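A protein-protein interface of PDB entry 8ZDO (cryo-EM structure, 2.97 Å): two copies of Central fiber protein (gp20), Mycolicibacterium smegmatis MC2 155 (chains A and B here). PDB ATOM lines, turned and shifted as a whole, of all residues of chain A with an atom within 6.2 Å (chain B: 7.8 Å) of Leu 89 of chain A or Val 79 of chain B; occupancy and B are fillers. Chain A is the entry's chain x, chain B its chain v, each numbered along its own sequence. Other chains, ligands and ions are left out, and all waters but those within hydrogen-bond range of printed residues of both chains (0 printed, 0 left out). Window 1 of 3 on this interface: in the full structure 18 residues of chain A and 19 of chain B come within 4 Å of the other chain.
The guanidinium group (NH1) of Arg 96 of chain B sits close to the indole nitrogen (NE1) of Trp 97 of chain A (3.1 Å).
O of Ala 82 of chain B lies within hydrogen-bond range of OG1 of Thr 80 of chain B (3.0 Å). The backbone carbonyl oxygen of Gln 90 of chain A lies within hydrogen-bond range of the side-chain hydroxyl of Thr 94 of chain A.
Among the printed residues, pairs that only touch across the chains: Leu 86 of chain A with Leu 74 of chain B (3.6 Å), Leu 86 of chain A with Ile 75 of chain B (3.6 Å), Leu 86 of chain A with Ala 78 of chain B (3.7 Å), Leu 89 of chain A with Ala 78 of chain B (3.8 Å), Leu 89 of chain A with Val 79 of chain B (3.7 Å), Gln 90 of chain A with Ala 78 of chain B (3.7 Å), Leu 93 of chain A with Ala 78 of chain B (3.98 Å), Leu 93 of chain A with Val 79 of chain B (3.6 Å), Trp 97 of chain A with Val 79 of chain B (3.1 Å), Trp 97 of chain A with Thr 80 of chain B (3.8 Å) and Trp 97 of chain A with Phe 92 of chain B (3.4 Å).
Of the printed residues of chain B, Leu 86 of chain A touches Leu 74, Ile 75 and Ala 78. Of the printed residues of chain B, Leu 89 of chain A touches Ala 78 and Val 79. Ala 91 of chain A touches none of the printed residues of chain B. Of the printed residues of chain B, Leu 93 of chain A touches Ala 78 and Val 79. Of the printed residues of chain A, Leu 74 of chain B touches Leu 86. Of the printed residues of chain A, Ile 75 of chain B touches Leu 86 (3.6 Å). Gln 77 of chain B touches none of the printed residues of chain A. Val 79 of chain B touches just these residues of chain A: Leu 89 (3.7 Å), Leu 93 (3.6 Å) and Trp 97 (3.1 Å). Printed residues of chain A within 4 Å of Arg 96 of chain B: Trp 97. The nearest residue of chain B that does not touch Leu 89 of chain A is Ile 75 of chain B (5.5 Å). The nearest residue of chain A that does not touch Val 79 of chain B is Gln 90 of chain A (5.8 Å).
Of the 17 printed residues of chain B, 7 touch a printed residue of chain A. Printed residues of chain B that touch a printed residue of chain A: Leu 74, Ile 75, Ala 78, Val 79, Thr 80, Phe 92 and Arg 96. Of the 17 printed residues of chain A, 5 touch a printed residue of chain B. Among the printed residues, no Asp or Glu carboxylate lies within 4 Å of a Lys or Arg side-chain nitrogen of the other chain.
Leu 89 of chain A touches Val 79 of chain B, but with the chains exchanged Val 79 of chain A does not touch Leu 89 of chain B (8.9 Å). Leu 93 of chain A touches Val 79 of chain B, but with the chains exchanged Val 79 of chain A does not touch Leu 93 of chain B (8.1 Å). Positions printed for both chains: 72, 75, 76, 79, 80, 88, 89, 90, 92 and 93. Of the 12 pairs that touch across the chains among the printed residues, none has its exchanged pair printed and touching as well.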
ATOM      1  N   VAL A  72       9.124  13.849  36.922  1.00  0.00           N
ATOM      2  CA  VAL A  72       9.884  13.910  35.676  1.00  0.00           C
ATOM      3  C   VAL A  72      10.517  12.562  35.377  1.00  0.00           C
ATOM      4  O   VAL A  72      10.518  12.099  34.229  1.00  0.00           O
ATOM      5  CB  VAL A  72      10.947  15.023  35.749  1.00  0.00           C
ATOM      6  CG1 VAL A  72      11.933  14.892  34.603  1.00  0.00           C
ATOM      7  CG2 VAL A  72      10.293  16.384  35.723  1.00  0.00           C
ATOM      8  N   ILE A  75       7.829  10.355  34.043  1.00  0.00           N
ATOM      9  CA  ILE A  75       7.512  10.693  32.656  1.00  0.00           C
ATOM     10  C   ILE A  75       8.559  10.112  31.716  1.00  0.00           C
ATOM     11  O   ILE A  75       8.232   9.541  30.664  1.00  0.00           O
ATOM     12  CB  ILE A  75       7.396  12.221  32.493  1.00  0.00           C
ATOM     13  CG1 ILE A  75       6.142  12.744  33.193  1.00  0.00           C
ATOM     14  CG2 ILE A  75       7.384  12.602  31.024  1.00  0.00           C
ATOM     15  CD1 ILE A  75       4.855  12.349  32.513  1.00  0.00           C
ATOM     16  N   VAL A  76       9.835  10.252  32.079  1.00  0.00           N
ATOM     17  CA  VAL A  76      10.912   9.723  31.247  1.00  0.00           C
ATOM     18  C   VAL A  76      10.803   8.208  31.138  1.00  0.00           C
ATOM     19  O   VAL A  76      10.970   7.638  30.055  1.00  0.00           O
ATOM     20  CB  VAL A  76      12.282  10.154  31.804  1.00  0.00           C
ATOM     21  CG1 VAL A  76      13.402   9.436  31.075  1.00  0.00           C
ATOM     22  CG2 VAL A  76      12.451  11.660  31.692  1.00  0.00           C
ATOM     23  N   VAL A  79       7.828   7.288  28.785  1.00  0.00           N
ATOM     24  CA  VAL A  79       8.000   7.515  27.353  1.00  0.00           C
ATOM     25  C   VAL A  79       9.132   6.657  26.791  1.00  0.00           C
ATOM     26  O   VAL A  79       9.036   6.146  25.669  1.00  0.00           O
ATOM     27  CB  VAL A  79       8.215   9.012  27.063  1.00  0.00           C
ATOM     28  CG1 VAL A  79       7.007   9.815  27.518  1.00  0.00           C
ATOM     29  CG2 VAL A  79       9.471   9.520  27.737  1.00  0.00           C
ATOM     30  N   THR A  80      10.213   6.480  27.546  1.00  0.00           N
ATOM     31  CA  THR A  80      11.362   5.699  27.116  1.00  0.00           C
ATOM     32  C   THR A  80      11.738   4.717  28.215  1.00  0.00           C
ATOM     33  O   THR A  80      11.562   4.995  29.403  1.00  0.00           O
ATOM     34  CB  THR A  80      12.576   6.586  26.790  1.00  0.00           C
ATOM     35  OG1 THR A  80      13.188   7.028  28.008  1.00  0.00           O
ATOM     36  CG2 THR A  80      12.158   7.799  25.973  1.00  0.00           C
ATOM     37  N   GLY A  84      15.961   8.409  33.516  1.00  0.00           N
ATOM     38  CA  GLY A  84      16.868   9.533  33.465  1.00  0.00           C
ATOM     39  C   GLY A  84      16.106  10.842  33.525  1.00  0.00           C
ATOM     40  O   GLY A  84      14.906  10.875  33.797  1.00  0.00           O
ATOM     41  N   GLY A  85      16.839  11.921  33.264  1.00  0.00           N
ATOM     42  CA  GLY A  85      16.291  13.257  33.319  1.00  0.00           C
ATOM     43  C   GLY A  85      15.697  13.702  31.998  1.00  0.00           C
ATOM     44  O   GLY A  85      15.579  12.941  31.034  1.00  0.00           O
ATOM     45  N   LEU A  86      15.308  14.978  31.964  1.00  0.00           N
ATOM     46  CA  LEU A  86      14.766  15.556  30.743  1.00  0.00           C
ATOM     47  C   LEU A  86      15.796  15.529  29.623  1.00  0.00           C
ATOM     48  O   LEU A  86      15.449  15.332  28.452  1.00  0.00           O
ATOM     49  CB  LEU A  86      14.297  16.984  31.010  1.00  0.00           C
ATOM     50  CG  LEU A  86      13.064  17.440  30.236  1.00  0.00           C
ATOM     51  CD1 LEU A  86      11.871  16.580  30.600  1.00  0.00           C
ATOM     52  CD2 LEU A  86      12.780  18.903  30.515  1.00  0.00           C
ATOM     53  N   THR A  87      17.071  15.729  29.964  1.00  0.00           N
ATOM     54  CA  THR A  87      18.129  15.632  28.966  1.00  0.00           C
ATOM     55  C   THR A  87      18.217  14.224  28.395  1.00  0.00           C
ATOM     56  O   THR A  87      18.403  14.050  27.187  1.00  0.00           O
ATOM     57  CB  THR A  87      19.467  16.045  29.577  1.00  0.00           C
ATOM     58  OG1 THR A  87      19.770  15.194  30.690  1.00  0.00           O
ATOM     59  CG2 THR A  87      19.414  17.491  30.050  1.00  0.00           C
ATOM     60  N   ASP A  88      18.092  13.206  29.250  1.00  0.00           N
ATOM     61  CA  ASP A  88      18.095  11.826  28.769  1.00  0.00           C
ATOM     62  C   ASP A  88      16.899  11.559  27.862  1.00  0.00           C
ATOM     63  O   ASP A  88      17.029  10.883  26.832  1.00  0.00           O
ATOM     64  CB  ASP A  88      18.101  10.861  29.953  1.00  0.00           C
ATOM     65  CG  ASP A  88      18.299   9.417  29.532  1.00  0.00           C
ATOM     66  OD1 ASP A  88      18.747   9.182  28.389  1.00  0.00           O
ATOM     67  OD2 ASP A  88      18.006   8.517  30.346  1.00  0.00           O
ATOM     68  N   LEU A  89      15.726  12.070  28.237  1.00  0.00           N
ATOM     69  CA  LEU A  89      14.545  11.935  27.389  1.00  0.00           C
ATOM     70  C   LEU A  89      14.788  12.557  26.019  1.00  0.00           C
ATOM     71  O   LEU A  89      14.503  11.946  24.981  1.00  0.00           O
ATOM     72  CB  LEU A  89      13.343  12.587  28.077  1.00  0.00           C
ATOM     73  CG  LEU A  89      11.934  12.521  27.480  1.00  0.00           C
ATOM     74  CD1 LEU A  89      10.908  12.626  28.590  1.00  0.00           C
ATOM     75  CD2 LEU A  89      11.706  13.634  26.476  1.00  0.00           C
ATOM     76  N   GLN A  90      15.326  13.778  26.004  1.00  0.00           N
ATOM     77  CA  GLN A  90      15.595  14.465  24.746  1.00  0.00           C
ATOM     78  C   GLN A  90      16.620  13.710  23.912  1.00  0.00           C
ATOM     79  O   GLN A  90      16.476  13.604  22.690  1.00  0.00           O
ATOM     80  CB  GLN A  90      16.074  15.891  25.022  1.00  0.00           C
ATOM     81  CG  GLN A  90      16.823  16.531  23.871  1.00  0.00           C
ATOM     82  CD  GLN A  90      17.285  17.938  24.192  1.00  0.00           C
ATOM     83  OE1 GLN A  90      17.040  18.449  25.284  1.00  0.00           O
ATOM     84  NE2 GLN A  90      17.955  18.574  23.236  1.00  0.00           N
ATOM     85  N   ALA A  91      17.660  13.176  24.555  1.00  0.00           N
ATOM     86  CA  ALA A  91      18.691  12.443  23.827  1.00  0.00           C
ATOM     87  C   ALA A  91      18.127  11.178  23.195  1.00  0.00           C
ATOM     88  O   ALA A  91      18.406  10.875  22.027  1.00  0.00           O
ATOM     89  CB  ALA A  91      19.852  12.108  24.765  1.00  0.00           C
ATOM     90  N   PHE A  92      17.330  10.420  23.955  1.00  0.00           N
ATOM     91  CA  PHE A  92      16.738   9.208  23.399  1.00  0.00           C
ATOM     92  C   PHE A  92      15.795   9.538  22.250  1.00  0.00           C
ATOM     93  O   PHE A  92      15.802   8.858  21.215  1.00  0.00           O
ATOM     94  CB  PHE A  92      16.004   8.424  24.486  1.00  0.00           C
ATOM     95  CG  PHE A  92      15.580   7.046  24.055  1.00  0.00           C
ATOM     96  CD1 PHE A  92      14.347   6.839  23.457  1.00  0.00           C
ATOM     97  CD2 PHE A  92      16.415   5.958  24.243  1.00  0.00           C
ATOM     98  CE1 PHE A  92      13.956   5.577  23.060  1.00  0.00           C
ATOM     99  CE2 PHE A  92      16.030   4.692  23.847  1.00  0.00           C
ATOM    100  CZ  PHE A  92      14.798   4.502  23.254  1.00  0.00           C
ATOM    101  N   LEU A  93      14.977  10.582  22.411  1.00  0.00           N
ATOM    102  CA  LEU A  93      14.061  10.959  21.342  1.00  0.00           C
ATOM    103  C   LEU A  93      14.818  11.426  20.105  1.00  0.00           C
ATOM    104  O   LEU A  93      14.420  11.119  18.978  1.00  0.00           O
ATOM    105  CB  LEU A  93      13.089  12.032  21.831  1.00  0.00           C
ATOM    106  CG  LEU A  93      11.802  11.473  22.441  1.00  0.00           C
ATOM    107  CD1 LEU A  93      10.997  12.566  23.105  1.00  0.00           C
ATOM    108  CD2 LEU A  93      10.966  10.765  21.388  1.00  0.00           C
ATOM    109  N   THR A  94      15.915  12.162  20.290  1.00  0.00           N
ATOM    110  CA  THR A  94      16.711  12.604  19.149  1.00  0.00           C
ATOM    111  C   THR A  94      17.349  11.424  18.426  1.00  0.00           C
ATOM    112  O   THR A  94      17.358  11.378  17.189  1.00  0.00           O
ATOM    113  CB  THR A  94      17.783  13.593  19.608  1.00  0.00           C
ATOM    114  OG1 THR A  94      17.181  14.622  20.403  1.00  0.00           O
ATOM    115  CG2 THR A  94      18.474  14.227  18.408  1.00  0.00           C
ATOM    116  N   TRP A  97      14.657   9.616  16.568  1.00  0.00           N
ATOM    117  CA  TRP A  97      14.256  10.422  15.419  1.00  0.00           C
ATOM    118  C   TRP A  97      15.258  10.297  14.281  1.00  0.00           C
ATOM    119  O   TRP A  97      14.870  10.218  13.111  1.00  0.00           O
ATOM    120  CB  TRP A  97      14.104  11.885  15.829  1.00  0.00           C
ATOM    121  CG  TRP A  97      12.821  12.191  16.525  1.00  0.00           C
ATOM    122  CD1 TRP A  97      11.813  11.320  16.811  1.00  0.00           C
ATOM    123  CD2 TRP A  97      12.407  13.465  17.029  1.00  0.00           C
ATOM    124  NE1 TRP A  97      10.795  11.973  17.461  1.00  0.00           N
ATOM    125  CE2 TRP A  97      11.135  13.292  17.606  1.00  0.00           C
ATOM    126  CE3 TRP A  97      12.989  14.737  17.047  1.00  0.00           C
ATOM    127  CZ2 TRP A  97      10.435  14.341  18.195  1.00  0.00           C
ATOM    128  CZ3 TRP A  97      12.292  15.776  17.632  1.00  0.00           C
ATOM    129  CH2 TRP A  97      11.030  15.572  18.199  1.00  0.00           C
ATOM    130  N   VAL B  72       5.974  22.728  31.676  1.00  0.00           N
ATOM    131  CA  VAL B  72       5.282  22.301  30.463  1.00  0.00           C
ATOM    132  C   VAL B  72       6.089  22.693  29.235  1.00  0.00           C
ATOM    133  O   VAL B  72       6.242  21.905  28.293  1.00  0.00           O
ATOM    134  CB  VAL B  72       3.864  22.898  30.412  1.00  0.00           C
ATOM    135  CG1 VAL B  72       3.219  22.621  29.064  1.00  0.00           C
ATOM    136  CG2 VAL B  72       3.015  22.339  31.525  1.00  0.00           C
ATOM    137  N   THR B  73       6.610  23.921  29.225  1.00  0.00           N
ATOM    138  CA  THR B  73       7.448  24.351  28.109  1.00  0.00           C
ATOM    139  C   THR B  73       8.686  23.471  27.983  1.00  0.00           C
ATOM    140  O   THR B  73       9.120  23.155  26.871  1.00  0.00           O
ATOM    141  CB  THR B  73       7.855  25.815  28.274  1.00  0.00           C
ATOM    142  OG1 THR B  73       8.731  25.946  29.399  1.00  0.00           O
ATOM    143  CG2 THR B  73       6.630  26.693  28.475  1.00  0.00           C
ATOM    144  N   LEU B  74       9.274  23.076  29.112  1.00  0.00           N
ATOM    145  CA  LEU B  74      10.440  22.199  29.083  1.00  0.00           C
ATOM    146  C   LEU B  74      10.092  20.826  28.519  1.00  0.00           C
ATOM    147  O   LEU B  74      10.870  20.250  27.754  1.00  0.00           O
ATOM    148  CB  LEU B  74      11.034  22.066  30.483  1.00  0.00           C
ATOM    149  CG  LEU B  74      11.760  23.292  31.036  1.00  0.00           C
ATOM    150  CD1 LEU B  74      12.700  22.884  32.155  1.00  0.00           C
ATOM    151  CD2 LEU B  74      12.516  24.017  29.936  1.00  0.00           C
ATOM    152  N   ILE B  75       8.935  20.284  28.896  1.00  0.00           N
ATOM    153  CA  ILE B  75       8.491  19.010  28.331  1.00  0.00           C
ATOM    154  C   ILE B  75       8.306  19.137  26.825  1.00  0.00           C
ATOM    155  O   ILE B  75       8.701  18.251  26.052  1.00  0.00           O
ATOM    156  CB  ILE B  75       7.195  18.543  29.021  1.00  0.00           C
ATOM    157  CG1 ILE B  75       7.459  18.204  30.488  1.00  0.00           C
ATOM    158  CG2 ILE B  75       6.603  17.349  28.295  1.00  0.00           C
ATOM    159  CD1 ILE B  75       8.257  16.939  30.689  1.00  0.00           C
ATOM    160  N   VAL B  76       7.699  20.241  26.386  1.00  0.00           N
ATOM    161  CA  VAL B  76       7.483  20.462  24.959  1.00  0.00           C
ATOM    162  C   VAL B  76       8.815  20.566  24.227  1.00  0.00           C
ATOM    163  O   VAL B  76       8.978  20.026  23.130  1.00  0.00           O
ATOM    164  CB  VAL B  76       6.616  21.715  24.736  1.00  0.00           C
ATOM    165  CG1 VAL B  76       6.504  22.027  23.255  1.00  0.00           C
ATOM    166  CG2 VAL B  76       5.238  21.518  25.344  1.00  0.00           C
ATOM    167  N   GLN B  77       9.785  21.264  24.818  1.00  0.00           N
ATOM    168  CA  GLN B  77      11.095  21.392  24.187  1.00  0.00           C
ATOM    169  C   GLN B  77      11.851  20.070  24.187  1.00  0.00           C
ATOM    170  O   GLN B  77      12.660  19.817  23.287  1.00  0.00           O
ATOM    171  CB  GLN B  77      11.913  22.473  24.894  1.00  0.00           C
ATOM    172  CG  GLN B  77      13.274  22.737  24.274  1.00  0.00           C
ATOM    173  CD  GLN B  77      13.176  23.299  22.870  1.00  0.00           C
ATOM    174  OE1 GLN B  77      12.347  24.164  22.593  1.00  0.00           O
ATOM    175  NE2 GLN B  77      14.023  22.806  21.975  1.00  0.00           N
ATOM    176  N   ALA B  78      11.607  19.218  25.183  1.00  0.00           N
ATOM    177  CA  ALA B  78      12.298  17.937  25.243  1.00  0.00           C
ATOM    178  C   ALA B  78      11.749  16.961  24.213  1.00  0.00           C
ATOM    179  O   ALA B  78      12.514  16.219  23.584  1.00  0.00           O
ATOM    180  CB  ALA B  78      12.192  17.349  26.649  1.00  0.00           C
ATOM    181  N   VAL B  79      10.426  16.941  24.022  1.00  0.00           N
ATOM    182  CA  VAL B  79       9.836  15.992  23.078  1.00  0.00           C
ATOM    183  C   VAL B  79       9.656  16.565  21.679  1.00  0.00           C
ATOM    184  O   VAL B  79       9.330  15.810  20.751  1.00  0.00           O
ATOM    185  CB  VAL B  79       8.468  15.477  23.564  1.00  0.00           C
ATOM    186  CG1 VAL B  79       8.606  14.776  24.906  1.00  0.00           C
ATOM    187  CG2 VAL B  79       7.474  16.611  23.638  1.00  0.00           C
ATOM    188  N   THR B  80       9.841  17.871  21.498  1.00  0.00           N
ATOM    189  CA  THR B  80       9.666  18.532  20.212  1.00  0.00           C
ATOM    190  C   THR B  80      10.748  19.587  20.053  1.00  0.00           C
ATOM    191  O   THR B  80      11.180  20.203  21.030  1.00  0.00           O
ATOM    192  CB  THR B  80       8.291  19.212  20.077  1.00  0.00           C
ATOM    193  OG1 THR B  80       8.216  20.319  20.984  1.00  0.00           O
ATOM    194  CG2 THR B  80       7.156  18.246  20.382  1.00  0.00           C
ATOM    195  N   GLY B  81      11.175  19.803  18.810  1.00  0.00           N
ATOM    196  CA  GLY B  81      12.173  20.829  18.558  1.00  0.00           C
ATOM    197  C   GLY B  81      11.658  22.229  18.834  1.00  0.00           C
ATOM    198  O   GLY B  81      12.349  23.045  19.452  1.00  0.00           O
ATOM    199  N   ALA B  82      10.443  22.527  18.391  1.00  0.00           N
ATOM    200  CA  ALA B  82       9.890  23.868  18.528  1.00  0.00           C
ATOM    201  C   ALA B  82       9.343  24.072  19.936  1.00  0.00           C
ATOM    202  O   ALA B  82       8.506  23.280  20.384  1.00  0.00           O
ATOM    203  CB  ALA B  82       8.790  24.097  17.501  1.00  0.00           C
ATOM    204  N   ASP B  88       0.977  23.024  21.198  1.00  0.00           N
ATOM    205  CA  ASP B  88       2.079  22.898  20.249  1.00  0.00           C
ATOM    206  C   ASP B  88       2.690  21.502  20.299  1.00  0.00           C
ATOM    207  O   ASP B  88       3.018  20.919  19.257  1.00  0.00           O
ATOM    208  CB  ASP B  88       3.139  23.960  20.541  1.00  0.00           C
ATOM    209  CG  ASP B  88       4.082  24.187  19.373  1.00  0.00           C
ATOM    210  OD1 ASP B  88       4.015  23.424  18.387  1.00  0.00           O
ATOM    211  OD2 ASP B  88       4.895  25.133  19.446  1.00  0.00           O
ATOM    212  N   LEU B  89       2.863  20.960  21.507  1.00  0.00           N
ATOM    213  CA  LEU B  89       3.359  19.594  21.652  1.00  0.00           C
ATOM    214  C   LEU B  89       2.447  18.610  20.931  1.00  0.00           C
ATOM    215  O   LEU B  89       2.912  17.746  20.174  1.00  0.00           O
ATOM    216  CB  LEU B  89       3.465  19.246  23.139  1.00  0.00           C
ATOM    217  CG  LEU B  89       3.910  17.864  23.626  1.00  0.00           C
ATOM    218  CD1 LEU B  89       4.542  17.992  24.999  1.00  0.00           C
ATOM    219  CD2 LEU B  89       2.750  16.889  23.689  1.00  0.00           C
ATOM    220  N   GLN B  90       1.139  18.728  21.164  1.00  0.00           N
ATOM    221  CA  GLN B  90       0.181  17.828  20.533  1.00  0.00           C
ATOM    222  C   GLN B  90       0.210  17.972  19.018  1.00  0.00           C
ATOM    223  O   GLN B  90       0.128  16.975  18.295  1.00  0.00           O
ATOM    224  CB  GLN B  90      -1.223  18.094  21.075  1.00  0.00           C
ATOM    225  CG  GLN B  90      -2.337  17.462  20.262  1.00  0.00           C
ATOM    226  CD  GLN B  90      -2.989  18.440  19.308  1.00  0.00           C
ATOM    227  OE1 GLN B  90      -3.096  19.630  19.600  1.00  0.00           O
ATOM    228  NE2 GLN B  90      -3.423  17.943  18.155  1.00  0.00           N
ATOM    229  N   PHE B  92       2.766  18.976  17.079  1.00  0.00           N
ATOM    230  CA  PHE B  92       3.983  18.380  16.536  1.00  0.00           C
ATOM    231  C   PHE B  92       3.907  16.859  16.564  1.00  0.00           C
ATOM    232  O   PHE B  92       4.313  16.192  15.605  1.00  0.00           O
ATOM    233  CB  PHE B  92       5.210  18.865  17.305  1.00  0.00           C
ATOM    234  CG  PHE B  92       6.516  18.394  16.722  1.00  0.00           C
ATOM    235  CD1 PHE B  92       7.074  17.187  17.111  1.00  0.00           C
ATOM    236  CD2 PHE B  92       7.180  19.155  15.776  1.00  0.00           C
ATOM    237  CE1 PHE B  92       8.269  16.753  16.574  1.00  0.00           C
ATOM    238  CE2 PHE B  92       8.377  18.727  15.235  1.00  0.00           C
ATOM    239  CZ  PHE B  92       8.922  17.524  15.635  1.00  0.00           C
ATOM    240  N   LEU B  93       3.391  16.289  17.655  1.00  0.00           N
ATOM    241  CA  LEU B  93       3.285  14.837  17.727  1.00  0.00           C
ATOM    242  C   LEU B  93       2.273  14.305  16.720  1.00  0.00           C
ATOM    243  O   LEU B  93       2.475  13.232  16.139  1.00  0.00           O
ATOM    244  CB  LEU B  93       2.923  14.405  19.148  1.00  0.00           C
ATOM    245  CG  LEU B  93       4.142  14.097  20.020  1.00  0.00           C
ATOM    246  CD1 LEU B  93       3.769  14.086  21.487  1.00  0.00           C
ATOM    247  CD2 LEU B  93       4.773  12.776  19.612  1.00  0.00           C
ATOM    248  N   ARG B  96       3.987  14.295  13.418  1.00  0.00           N
ATOM    249  CA  ARG B  96       4.932  13.186  13.357  1.00  0.00           C
ATOM    250  C   ARG B  96       4.219  11.858  13.125  1.00  0.00           C
ATOM    251  O   ARG B  96       4.659  11.047  12.305  1.00  0.00           O
ATOM    252  CB  ARG B  96       5.764  13.132  14.637  1.00  0.00           C
ATOM    253  CG  ARG B  96       7.070  13.900  14.557  1.00  0.00           C
ATOM    254  CD  ARG B  96       8.093  13.321  15.515  1.00  0.00           C
ATOM    255  NE  ARG B  96       8.278  11.895  15.282  1.00  0.00           N
ATOM    256  CZ  ARG B  96       8.104  10.956  16.201  1.00  0.00           C
ATOM    257  NH1 ARG B  96       7.779  11.258  17.447  1.00  0.00           N
ATOM    258  NH2 ARG B  96       8.255   9.680  15.860  1.00  0.00           N
